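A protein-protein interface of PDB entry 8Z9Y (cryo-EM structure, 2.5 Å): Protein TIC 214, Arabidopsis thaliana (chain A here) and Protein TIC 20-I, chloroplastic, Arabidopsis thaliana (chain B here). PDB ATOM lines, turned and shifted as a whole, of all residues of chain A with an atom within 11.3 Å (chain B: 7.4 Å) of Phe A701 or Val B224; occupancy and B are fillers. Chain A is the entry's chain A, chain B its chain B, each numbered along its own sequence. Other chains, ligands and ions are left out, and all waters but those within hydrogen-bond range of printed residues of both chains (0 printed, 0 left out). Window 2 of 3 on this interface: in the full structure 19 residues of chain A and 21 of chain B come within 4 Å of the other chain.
O of Glu A699 is in hydrogen-bond range of N of Lys B228.
The backbone carbonyl oxygen (O) of Phe A700 lies within hydrogen-bond range of the backbone NH (N) of Lys B228 (3.1 Å).
The backbone NH of Gln A702 lies within hydrogen-bond range of the backbone carbonyl oxygen of Gly B223.
The backbone carbonyl oxygen of Gln A702 sits close to the backbone carbonyl oxygen of Leu B222, 3.0 Å away.
N of Trp A698 is in hydrogen-bond range of OE1 of Gln A702.
The side-chain amide nitrogen of Gln A702 is in hydrogen-bond range of the backbone carbonyl oxygen of Lys A704, 3.0 Å away.
Among the printed residues, pairs that only touch across the chains: Phe A701 with Gly B223, Phe A700 with Gly B227, Phe A679 with Trp B226, Gln A702 with Gly B227, Ala A703 with Leu B222, Gln A702 with Trp B226, Ile A697 with Trp B226, Ile A697 with Lys B228, Phe A700 with Phe B229, Ala A703 with Gly B223, Phe A701 with Val B224 and Ile A697 with Gly B227.
Phe A701 touches just these residues of chain B: Gly B223 (3.3 Å) and Val B224 (3.9 Å).
No residue of chain A comes within 4 Å of Met B220.
Gly B223 touches just these residues of chain A: Phe A701 (3.3 Å), Gln A702 (2.5 Å) and Ala A703 (3.8 Å).
Gly B227 touches just these residues of chain A: Ile A697 (3.9 Å), Phe A700 (3.4 Å) and Gln A702 (3.5 Å).
Gly B230 touches none of the printed residues of chain A.
Of the printed residues of chain B, Gln A702 touches Leu B222 (3.0 Å), Gly B223 (2.5 Å), Trp B226 (3.7 Å) and Gly B227 (3.5 Å).
Printed residues of chain A within 4 Å of Lys B228: Ile A697 (3.8 Å), Glu A699 (3.5 Å) and Phe A700 (3.1 Å).
Printed residues of chain B within 4 Å of Ala A703: Leu B222 (3.7 Å) and Gly B223 (3.8 Å).
Of the printed residues of chain B, Phe A679 touches Trp B226.
Tyr B225 touches none of the printed residues of chain A.
The nearest residue of chain A that does not touch Val B224 is Gln A702 (4.5 Å).
Along chain B the printed residues that touch a printed residue of chain A span positions 222 to 229.
Of the 14 printed residues of chain A, 7 touch a printed residue of chain B.
Among the printed residues, no Asp or Glu carboxylate lies within 4 Å of a Lys or Arg side-chain nitrogen of the other chain.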
ATOM      1  N   PHE A 679      28.536  17.311 -15.736  1.00  0.00           N
ATOM      2  CA  PHE A 679      27.662  16.146 -15.719  1.00  0.00           C
ATOM      3  C   PHE A 679      27.368  15.599 -17.109  1.00  0.00           C
ATOM      4  O   PHE A 679      26.964  14.437 -17.228  1.00  0.00           O
ATOM      5  CB  PHE A 679      26.337  16.481 -15.022  1.00  0.00           C
ATOM      6  CG  PHE A 679      26.466  16.692 -13.539  1.00  0.00           C
ATOM      7  CD1 PHE A 679      27.016  17.859 -13.034  1.00  0.00           C
ATOM      8  CD2 PHE A 679      26.033  15.722 -12.651  1.00  0.00           C
ATOM      9  CE1 PHE A 679      27.135  18.052 -11.670  1.00  0.00           C
ATOM     10  CE2 PHE A 679      26.149  15.910 -11.287  1.00  0.00           C
ATOM     11  CZ  PHE A 679      26.701  17.076 -10.796  1.00  0.00           C
ATOM     12  N   VAL A 696      25.993   7.665 -12.002  1.00  0.00           N
ATOM     13  CA  VAL A 696      24.630   7.661 -11.483  1.00  0.00           C
ATOM     14  C   VAL A 696      24.520   8.674 -10.351  1.00  0.00           C
ATOM     15  O   VAL A 696      25.518   9.181  -9.834  1.00  0.00           O
ATOM     16  CB  VAL A 696      24.202   6.265 -10.987  1.00  0.00           C
ATOM     17  CG1 VAL A 696      24.014   5.312 -12.155  1.00  0.00           C
ATOM     18  CG2 VAL A 696      25.233   5.721 -10.016  1.00  0.00           C
ATOM     19  N   ILE A 697      23.279   8.962  -9.970  1.00  0.00           N
ATOM     20  CA  ILE A 697      22.966   9.774  -8.800  1.00  0.00           C
ATOM     21  C   ILE A 697      22.444   8.813  -7.741  1.00  0.00           C
ATOM     22  O   ILE A 697      21.302   8.345  -7.814  1.00  0.00           O
ATOM     23  CB  ILE A 697      21.950  10.876  -9.117  1.00  0.00           C
ATOM     24  CG1 ILE A 697      22.447  11.745 -10.272  1.00  0.00           C
ATOM     25  CG2 ILE A 697      21.691  11.727  -7.885  1.00  0.00           C
ATOM     26  CD1 ILE A 697      23.700  12.526  -9.951  1.00  0.00           C
ATOM     27  N   TRP A 698      23.280   8.516  -6.746  1.00  0.00           N
ATOM     28  CA  TRP A 698      23.006   7.438  -5.803  1.00  0.00           C
ATOM     29  C   TRP A 698      22.329   7.916  -4.524  1.00  0.00           C
ATOM     30  O   TRP A 698      21.465   7.215  -3.988  1.00  0.00           O
ATOM     31  CB  TRP A 698      24.310   6.715  -5.457  1.00  0.00           C
ATOM     32  CG  TRP A 698      24.158   5.243  -5.213  1.00  0.00           C
ATOM     33  CD1 TRP A 698      24.419   4.575  -4.052  1.00  0.00           C
ATOM     34  CD2 TRP A 698      23.721   4.254  -6.153  1.00  0.00           C
ATOM     35  NE1 TRP A 698      24.167   3.234  -4.210  1.00  0.00           N
ATOM     36  CE2 TRP A 698      23.738   3.011  -5.491  1.00  0.00           C
ATOM     37  CE3 TRP A 698      23.313   4.299  -7.489  1.00  0.00           C
ATOM     38  CZ2 TRP A 698      23.364   1.824  -6.118  1.00  0.00           C
ATOM     39  CZ3 TRP A 698      22.943   3.120  -8.112  1.00  0.00           C
ATOM     40  CH2 TRP A 698      22.971   1.901  -7.425  1.00  0.00           C
ATOM     41  N   GLU A 699      22.696   9.091  -4.022  1.00  0.00           N
ATOM     42  CA  GLU A 699      22.280   9.536  -2.702  1.00  0.00           C
ATOM     43  C   GLU A 699      21.273  10.676  -2.805  1.00  0.00           C
ATOM     44  O   GLU A 699      21.074  11.270  -3.869  1.00  0.00           O
ATOM     45  CB  GLU A 699      23.493   9.979  -1.875  1.00  0.00           C
ATOM     46  CG  GLU A 699      23.296   9.910  -0.367  1.00  0.00           C
ATOM     47  CD  GLU A 699      23.347   8.490   0.162  1.00  0.00           C
ATOM     48  OE1 GLU A 699      24.463   7.954   0.330  1.00  0.00           O
ATOM     49  OE2 GLU A 699      22.269   7.908   0.406  1.00  0.00           O
ATOM     50  N   PHE A 700      20.626  10.960  -1.672  1.00  0.00           N
ATOM     51  CA  PHE A 700      19.692  12.078  -1.593  1.00  0.00           C
ATOM     52  C   PHE A 700      20.377  13.389  -1.958  1.00  0.00           C
ATOM     53  O   PHE A 700      19.874  14.160  -2.783  1.00  0.00           O
ATOM     54  CB  PHE A 700      19.108  12.158  -0.181  1.00  0.00           C
ATOM     55  CG  PHE A 700      17.624  12.370  -0.143  1.00  0.00           C
ATOM     56  CD1 PHE A 700      16.757  11.295  -0.226  1.00  0.00           C
ATOM     57  CD2 PHE A 700      17.095  13.642  -0.008  1.00  0.00           C
ATOM     58  CE1 PHE A 700      15.392  11.483  -0.182  1.00  0.00           C
ATOM     59  CE2 PHE A 700      15.728  13.838   0.034  1.00  0.00           C
ATOM     60  CZ  PHE A 700      14.876  12.757  -0.054  1.00  0.00           C
ATOM     61  N   PHE A 701      21.530  13.656  -1.351  1.00  0.00           N
ATOM     62  CA  PHE A 701      22.313  14.856  -1.612  1.00  0.00           C
ATOM     63  C   PHE A 701      23.577  14.463  -2.361  1.00  0.00           C
ATOM     64  O   PHE A 701      24.244  13.492  -1.991  1.00  0.00           O
ATOM     65  CB  PHE A 701      22.678  15.593  -0.313  1.00  0.00           C
ATOM     66  CG  PHE A 701      21.494  15.985   0.538  1.00  0.00           C
ATOM     67  CD1 PHE A 701      21.690  16.466   1.822  1.00  0.00           C
ATOM     68  CD2 PHE A 701      20.199  15.928   0.046  1.00  0.00           C
ATOM     69  CE1 PHE A 701      20.619  16.840   2.613  1.00  0.00           C
ATOM     70  CE2 PHE A 701      19.126  16.301   0.830  1.00  0.00           C
ATOM     71  CZ  PHE A 701      19.336  16.760   2.114  1.00  0.00           C
ATOM     72  N   GLN A 702      23.901  15.217  -3.408  1.00  0.00           N
ATOM     73  CA  GLN A 702      25.077  14.937  -4.219  1.00  0.00           C
ATOM     74  C   GLN A 702      25.473  16.197  -4.970  1.00  0.00           C
ATOM     75  O   GLN A 702      24.617  16.894  -5.522  1.00  0.00           O
ATOM     76  CB  GLN A 702      24.817  13.791  -5.202  1.00  0.00           C
ATOM     77  CG  GLN A 702      26.074  13.114  -5.711  1.00  0.00           C
ATOM     78  CD  GLN A 702      25.771  11.913  -6.581  1.00  0.00           C
ATOM     79  OE1 GLN A 702      24.764  11.233  -6.387  1.00  0.00           O
ATOM     80  NE2 GLN A 702      26.640  11.647  -7.547  1.00  0.00           N
ATOM     81  N   ALA A 703      26.777  16.480  -4.994  1.00  0.00           N
ATOM     82  CA  ALA A 703      27.296  17.674  -5.642  1.00  0.00           C
ATOM     83  C   ALA A 703      28.186  17.395  -6.842  1.00  0.00           C
ATOM     84  O   ALA A 703      28.350  18.288  -7.681  1.00  0.00           O
ATOM     85  CB  ALA A 703      28.082  18.532  -4.638  1.00  0.00           C
ATOM     86  N   LYS A 704      28.761  16.199  -6.954  1.00  0.00           N
ATOM     87  CA  LYS A 704      29.637  15.880  -8.073  1.00  0.00           C
ATOM     88  C   LYS A 704      29.202  14.588  -8.750  1.00  0.00           C
ATOM     89  O   LYS A 704      28.154  14.026  -8.415  1.00  0.00           O
ATOM     90  CB  LYS A 704      31.090  15.766  -7.606  1.00  0.00           C
ATOM     91  CG  LYS A 704      31.617  16.999  -6.894  1.00  0.00           C
ATOM     92  CD  LYS A 704      32.024  16.676  -5.466  1.00  0.00           C
ATOM     93  CE  LYS A 704      33.289  15.836  -5.432  1.00  0.00           C
ATOM     94  NZ  LYS A 704      33.438  15.108  -4.142  1.00  0.00           N
ATOM     95  N   VAL A 705      29.999  14.112  -9.701  1.00  0.00           N
ATOM     96  CA  VAL A 705      29.733  12.865 -10.408  1.00  0.00           C
ATOM     97  C   VAL A 705      30.609  11.779  -9.805  1.00  0.00           C
ATOM     98  O   VAL A 705      31.835  11.930  -9.729  1.00  0.00           O
ATOM     99  CB  VAL A 705      29.996  13.012 -11.915  1.00  0.00           C
ATOM    100  CG1 VAL A 705      29.591  11.747 -12.647  1.00  0.00           C
ATOM    101  CG2 VAL A 705      29.256  14.215 -12.468  1.00  0.00           C
ATOM    102  N   HIS A 706      29.987  10.685  -9.375  1.00  0.00           N
ATOM    103  CA  HIS A 706      30.697   9.584  -8.743  1.00  0.00           C
ATOM    104  C   HIS A 706      30.241   8.262  -9.337  1.00  0.00           C
ATOM    105  O   HIS A 706      29.068   8.099  -9.683  1.00  0.00           O
ATOM    106  CB  HIS A 706      30.469   9.568  -7.229  1.00  0.00           C
ATOM    107  CG  HIS A 706      30.971  10.790  -6.526  1.00  0.00           C
ATOM    108  ND1 HIS A 706      32.308  11.112  -6.460  1.00  0.00           N
ATOM    109  CD2 HIS A 706      30.314  11.764  -5.854  1.00  0.00           C
ATOM    110  CE1 HIS A 706      32.454  12.236  -5.780  1.00  0.00           C
ATOM    111  NE2 HIS A 706      31.259  12.651  -5.402  1.00  0.00           N
ATOM    112  N   PHE A 711      31.427   5.681  -4.653  1.00  0.00           N
ATOM    113  CA  PHE A 711      30.747   6.725  -3.894  1.00  0.00           C
ATOM    114  C   PHE A 711      30.710   6.410  -2.402  1.00  0.00           C
ATOM    115  O   PHE A 711      30.972   7.288  -1.573  1.00  0.00           O
ATOM    116  CB  PHE A 711      29.332   6.923  -4.436  1.00  0.00           C
ATOM    117  CG  PHE A 711      28.621   8.109  -3.854  1.00  0.00           C
ATOM    118  CD1 PHE A 711      29.325   9.241  -3.479  1.00  0.00           C
ATOM    119  CD2 PHE A 711      27.249   8.094  -3.685  1.00  0.00           C
ATOM    120  CE1 PHE A 711      28.673  10.334  -2.942  1.00  0.00           C
ATOM    121  CE2 PHE A 711      26.592   9.183  -3.150  1.00  0.00           C
ATOM    122  CZ  PHE A 711      27.305  10.304  -2.778  1.00  0.00           C
ATOM    123  N   ASP A 712      30.392   5.169  -2.040  1.00  0.00           N
ATOM    124  CA  ASP A 712      30.210   4.801  -0.635  1.00  0.00           C
ATOM    125  C   ASP A 712      31.539   4.384   0.000  1.00  0.00           C
ATOM    126  O   ASP A 712      31.685   3.302   0.566  1.00  0.00           O
ATOM    127  CB  ASP A 712      29.163   3.701  -0.509  1.00  0.00           C
ATOM    128  CG  ASP A 712      29.292   2.647  -1.590  1.00  0.00           C
ATOM    129  OD1 ASP A 712      30.165   2.802  -2.468  1.00  0.00           O
ATOM    130  OD2 ASP A 712      28.520   1.667  -1.561  1.00  0.00           O
ATOM    131  N   THR B 145      18.920  19.672 -14.318  1.00  0.00           N
ATOM    132  CA  THR B 145      19.122  18.623 -13.325  1.00  0.00           C
ATOM    133  C   THR B 145      18.168  17.457 -13.543  1.00  0.00           C
ATOM    134  O   THR B 145      18.496  16.316 -13.203  1.00  0.00           O
ATOM    135  CB  THR B 145      18.956  19.186 -11.913  1.00  0.00           C
ATOM    136  OG1 THR B 145      19.025  18.120 -10.960  1.00  0.00           O
ATOM    137  CG2 THR B 145      17.622  19.899 -11.774  1.00  0.00           C
ATOM    138  N   SER B 217      16.577  28.521  -6.690  1.00  0.00           N
ATOM    139  CA  SER B 217      17.260  27.262  -6.971  1.00  0.00           C
ATOM    140  C   SER B 217      18.772  27.446  -7.037  1.00  0.00           C
ATOM    141  O   SER B 217      19.519  26.650  -6.456  1.00  0.00           O
ATOM    142  CB  SER B 217      16.735  26.667  -8.277  1.00  0.00           C
ATOM    143  OG  SER B 217      17.300  27.329  -9.395  1.00  0.00           O
ATOM    144  N   MET B 220      20.500  27.863  -3.599  1.00  0.00           N
ATOM    145  CA  MET B 220      20.707  26.657  -2.813  1.00  0.00           C
ATOM    146  C   MET B 220      22.034  26.002  -3.198  1.00  0.00           C
ATOM    147  O   MET B 220      22.470  26.115  -4.348  1.00  0.00           O
ATOM    148  CB  MET B 220      19.563  25.668  -3.032  1.00  0.00           C
ATOM    149  CG  MET B 220      18.348  25.757  -2.088  1.00  0.00           C
ATOM    150  SD  MET B 220      18.566  25.894  -0.292  1.00  0.00           S
ATOM    151  CE  MET B 220      18.990  27.621  -0.043  1.00  0.00           C
ATOM    152  N   PRO B 221      22.694  25.320  -2.265  1.00  0.00           N
ATOM    153  CA  PRO B 221      23.962  24.657  -2.596  1.00  0.00           C
ATOM    154  C   PRO B 221      23.768  23.527  -3.598  1.00  0.00           C
ATOM    155  O   PRO B 221      22.697  22.923  -3.690  1.00  0.00           O
ATOM    156  CB  PRO B 221      24.450  24.125  -1.243  1.00  0.00           C
ATOM    157  CG  PRO B 221      23.221  24.066  -0.389  1.00  0.00           C
ATOM    158  CD  PRO B 221      22.372  25.213  -0.833  1.00  0.00           C
ATOM    159  N   LEU B 222      24.829  23.246  -4.359  1.00  0.00           N
ATOM    160  CA  LEU B 222      24.781  22.205  -5.379  1.00  0.00           C
ATOM    161  C   LEU B 222      24.657  20.802  -4.800  1.00  0.00           C
ATOM    162  O   LEU B 222      24.373  19.867  -5.556  1.00  0.00           O
ATOM    163  CB  LEU B 222      26.022  22.282  -6.271  1.00  0.00           C
ATOM    164  CG  LEU B 222      25.960  23.228  -7.470  1.00  0.00           C
ATOM    165  CD1 LEU B 222      26.251  24.654  -7.042  1.00  0.00           C
ATOM    166  CD2 LEU B 222      26.942  22.783  -8.540  1.00  0.00           C
ATOM    167  N   GLY B 223      24.871  20.629  -3.495  1.00  0.00           N
ATOM    168  CA  GLY B 223      24.733  19.308  -2.905  1.00  0.00           C
ATOM    169  C   GLY B 223      23.317  18.770  -2.995  1.00  0.00           C
ATOM    170  O   GLY B 223      23.108  17.580  -3.244  1.00  0.00           O
ATOM    171  N   VAL B 224      22.324  19.639  -2.796  1.00  0.00           N
ATOM    172  CA  VAL B 224      20.924  19.234  -2.861  1.00  0.00           C
ATOM    173  C   VAL B 224      20.282  19.546  -4.203  1.00  0.00           C
ATOM    174  O   VAL B 224      19.126  19.151  -4.429  1.00  0.00           O
ATOM    175  CB  VAL B 224      20.103  19.889  -1.729  1.00  0.00           C
ATOM    176  CG1 VAL B 224      20.834  19.759  -0.405  1.00  0.00           C
ATOM    177  CG2 VAL B 224      19.834  21.350  -2.051  1.00  0.00           C
ATOM    178  N   TYR B 225      20.984  20.238  -5.100  1.00  0.00           N
ATOM    179  CA  TYR B 225      20.421  20.547  -6.411  1.00  0.00           C
ATOM    180  C   TYR B 225      20.534  19.353  -7.352  1.00  0.00           C
ATOM    181  O   TYR B 225      19.528  18.854  -7.867  1.00  0.00           O
ATOM    182  CB  TYR B 225      21.117  21.774  -7.006  1.00  0.00           C
ATOM    183  CG  TYR B 225      20.666  22.106  -8.409  1.00  0.00           C
ATOM    184  CD1 TYR B 225      19.527  22.866  -8.626  1.00  0.00           C
ATOM    185  CD2 TYR B 225      21.380  21.664  -9.515  1.00  0.00           C
ATOM    186  CE1 TYR B 225      19.107  23.173  -9.904  1.00  0.00           C
ATOM    187  CE2 TYR B 225      20.968  21.965 -10.796  1.00  0.00           C
ATOM    188  CZ  TYR B 225      19.831  22.721 -10.984  1.00  0.00           C
ATOM    189  OH  TYR B 225      19.413  23.027 -12.257  1.00  0.00           O
ATOM    190  N   TRP B 226      21.757  18.882  -7.588  1.00  0.00           N
ATOM    191  CA  TRP B 226      21.990  17.737  -8.456  1.00  0.00           C
ATOM    192  C   TRP B 226      21.616  16.413  -7.804  1.00  0.00           C
ATOM    193  O   TRP B 226      21.656  15.378  -8.479  1.00  0.00           O
ATOM    194  CB  TRP B 226      23.455  17.700  -8.896  1.00  0.00           C
ATOM    195  CG  TRP B 226      23.849  18.853  -9.766  1.00  0.00           C
ATOM    196  CD1 TRP B 226      24.483  19.995  -9.374  1.00  0.00           C
ATOM    197  CD2 TRP B 226      23.635  18.978 -11.176  1.00  0.00           C
ATOM    198  NE1 TRP B 226      24.678  20.823 -10.452  1.00  0.00           N
ATOM    199  CE2 TRP B 226      24.166  20.221 -11.571  1.00  0.00           C
ATOM    200  CE3 TRP B 226      23.046  18.159 -12.144  1.00  0.00           C
ATOM    201  CZ2 TRP B 226      24.126  20.665 -12.890  1.00  0.00           C
ATOM    202  CZ3 TRP B 226      23.008  18.602 -13.454  1.00  0.00           C
ATOM    203  CH2 TRP B 226      23.545  19.842 -13.815  1.00  0.00           C
ATOM    204  N   GLY B 227      21.261  16.417  -6.525  1.00  0.00           N
ATOM    205  CA  GLY B 227      20.902  15.199  -5.835  1.00  0.00           C
ATOM    206  C   GLY B 227      19.568  14.645  -6.300  1.00  0.00           C
ATOM    207  O   GLY B 227      18.880  15.199  -7.160  1.00  0.00           O
ATOM    208  N   LYS B 228      19.198  13.510  -5.705  1.00  0.00           N
ATOM    209  CA  LYS B 228      17.985  12.805  -6.099  1.00  0.00           C
ATOM    210  C   LYS B 228      16.712  13.570  -5.758  1.00  0.00           C
ATOM    211  O   LYS B 228      15.639  13.194  -6.242  1.00  0.00           O
ATOM    212  CB  LYS B 228      17.951  11.424  -5.442  1.00  0.00           C
ATOM    213  CG  LYS B 228      17.298  10.348  -6.293  1.00  0.00           C
ATOM    214  CD  LYS B 228      17.455   8.976  -5.663  1.00  0.00           C
ATOM    215  CE  LYS B 228      16.407   8.008  -6.185  1.00  0.00           C
ATOM    216  NZ  LYS B 228      16.177   8.176  -7.646  1.00  0.00           N
ATOM    217  N   PHE B 229      16.800  14.620  -4.944  1.00  0.00           N
ATOM    218  CA  PHE B 229      15.638  15.432  -4.608  1.00  0.00           C
ATOM    219  C   PHE B 229      15.450  16.602  -5.565  1.00  0.00           C
ATOM    220  O   PHE B 229      14.319  16.892  -5.978  1.00  0.00           O
ATOM    221  CB  PHE B 229      15.762  15.951  -3.173  1.00  0.00           C
ATOM    222  CG  PHE B 229      14.712  16.955  -2.798  1.00  0.00           C
ATOM    223  CD1 PHE B 229      13.375  16.596  -2.750  1.00  0.00           C
ATOM    224  CD2 PHE B 229      15.060  18.260  -2.495  1.00  0.00           C
ATOM    225  CE1 PHE B 229      12.408  17.521  -2.404  1.00  0.00           C
ATOM    226  CE2 PHE B 229      14.099  19.188  -2.150  1.00  0.00           C
ATOM    227  CZ  PHE B 229      12.771  18.819  -2.104  1.00  0.00           C
ATOM    228  N   GLY B 230      16.542  17.278  -5.927  1.00  0.00           N
ATOM    229  CA  GLY B 230      16.429  18.441  -6.792  1.00  0.00           C
ATOM    230  C   GLY B 230      15.883  18.099  -8.164  1.00  0.00           C
ATOM    231  O   GLY B 230      15.027  18.808  -8.700  1.00  0.00           O
ATOM    232  N   MET B 231      16.369  17.004  -8.752  1.00  0.00           N
ATOM    233  CA  MET B 231      15.897  16.614 -10.076  1.00  0.00           C
ATOM    234  C   MET B 231      14.429  16.200 -10.041  1.00  0.00           C
ATOM    235  O   MET B 231      13.667  16.522 -10.962  1.00  0.00           O
ATOM    236  CB  MET B 231      16.783  15.501 -10.646  1.00  0.00           C
ATOM    237  CG  MET B 231      16.412  14.077 -10.257  1.00  0.00           C
ATOM    238  SD  MET B 231      17.703  12.894 -10.688  1.00  0.00           S
ATOM    239  CE  MET B 231      16.829  11.344 -10.494  1.00  0.00           C
ATOM    240  N   TRP B 234      12.425  19.335  -9.856  1.00  0.00           N
ATOM    241  CA  TRP B 234      12.481  20.185 -11.035  1.00  0.00           C
ATOM    242  C   TRP B 234      11.760  19.579 -12.230  1.00  0.00           C
ATOM    243  O   TRP B 234      11.194  20.325 -13.033  1.00  0.00           O
ATOM    244  CB  TRP B 234      13.933  20.495 -11.394  1.00  0.00           C
ATOM    245  CG  TRP B 234      14.359  21.834 -10.889  1.00  0.00           C
ATOM    246  CD1 TRP B 234      15.232  22.088  -9.873  1.00  0.00           C
ATOM    247  CD2 TRP B 234      13.891  23.108 -11.345  1.00  0.00           C
ATOM    248  NE1 TRP B 234      15.357  23.443  -9.686  1.00  0.00           N
ATOM    249  CE2 TRP B 234      14.542  24.091 -10.576  1.00  0.00           C
ATOM    250  CE3 TRP B 234      12.995  23.513 -12.338  1.00  0.00           C
ATOM    251  CZ2 TRP B 234      14.323  25.453 -10.766  1.00  0.00           C
ATOM    252  CZ3 TRP B 234      12.780  24.864 -12.526  1.00  0.00           C
ATOM    253  CH2 TRP B 234      13.439  25.818 -11.744  1.00  0.00           C
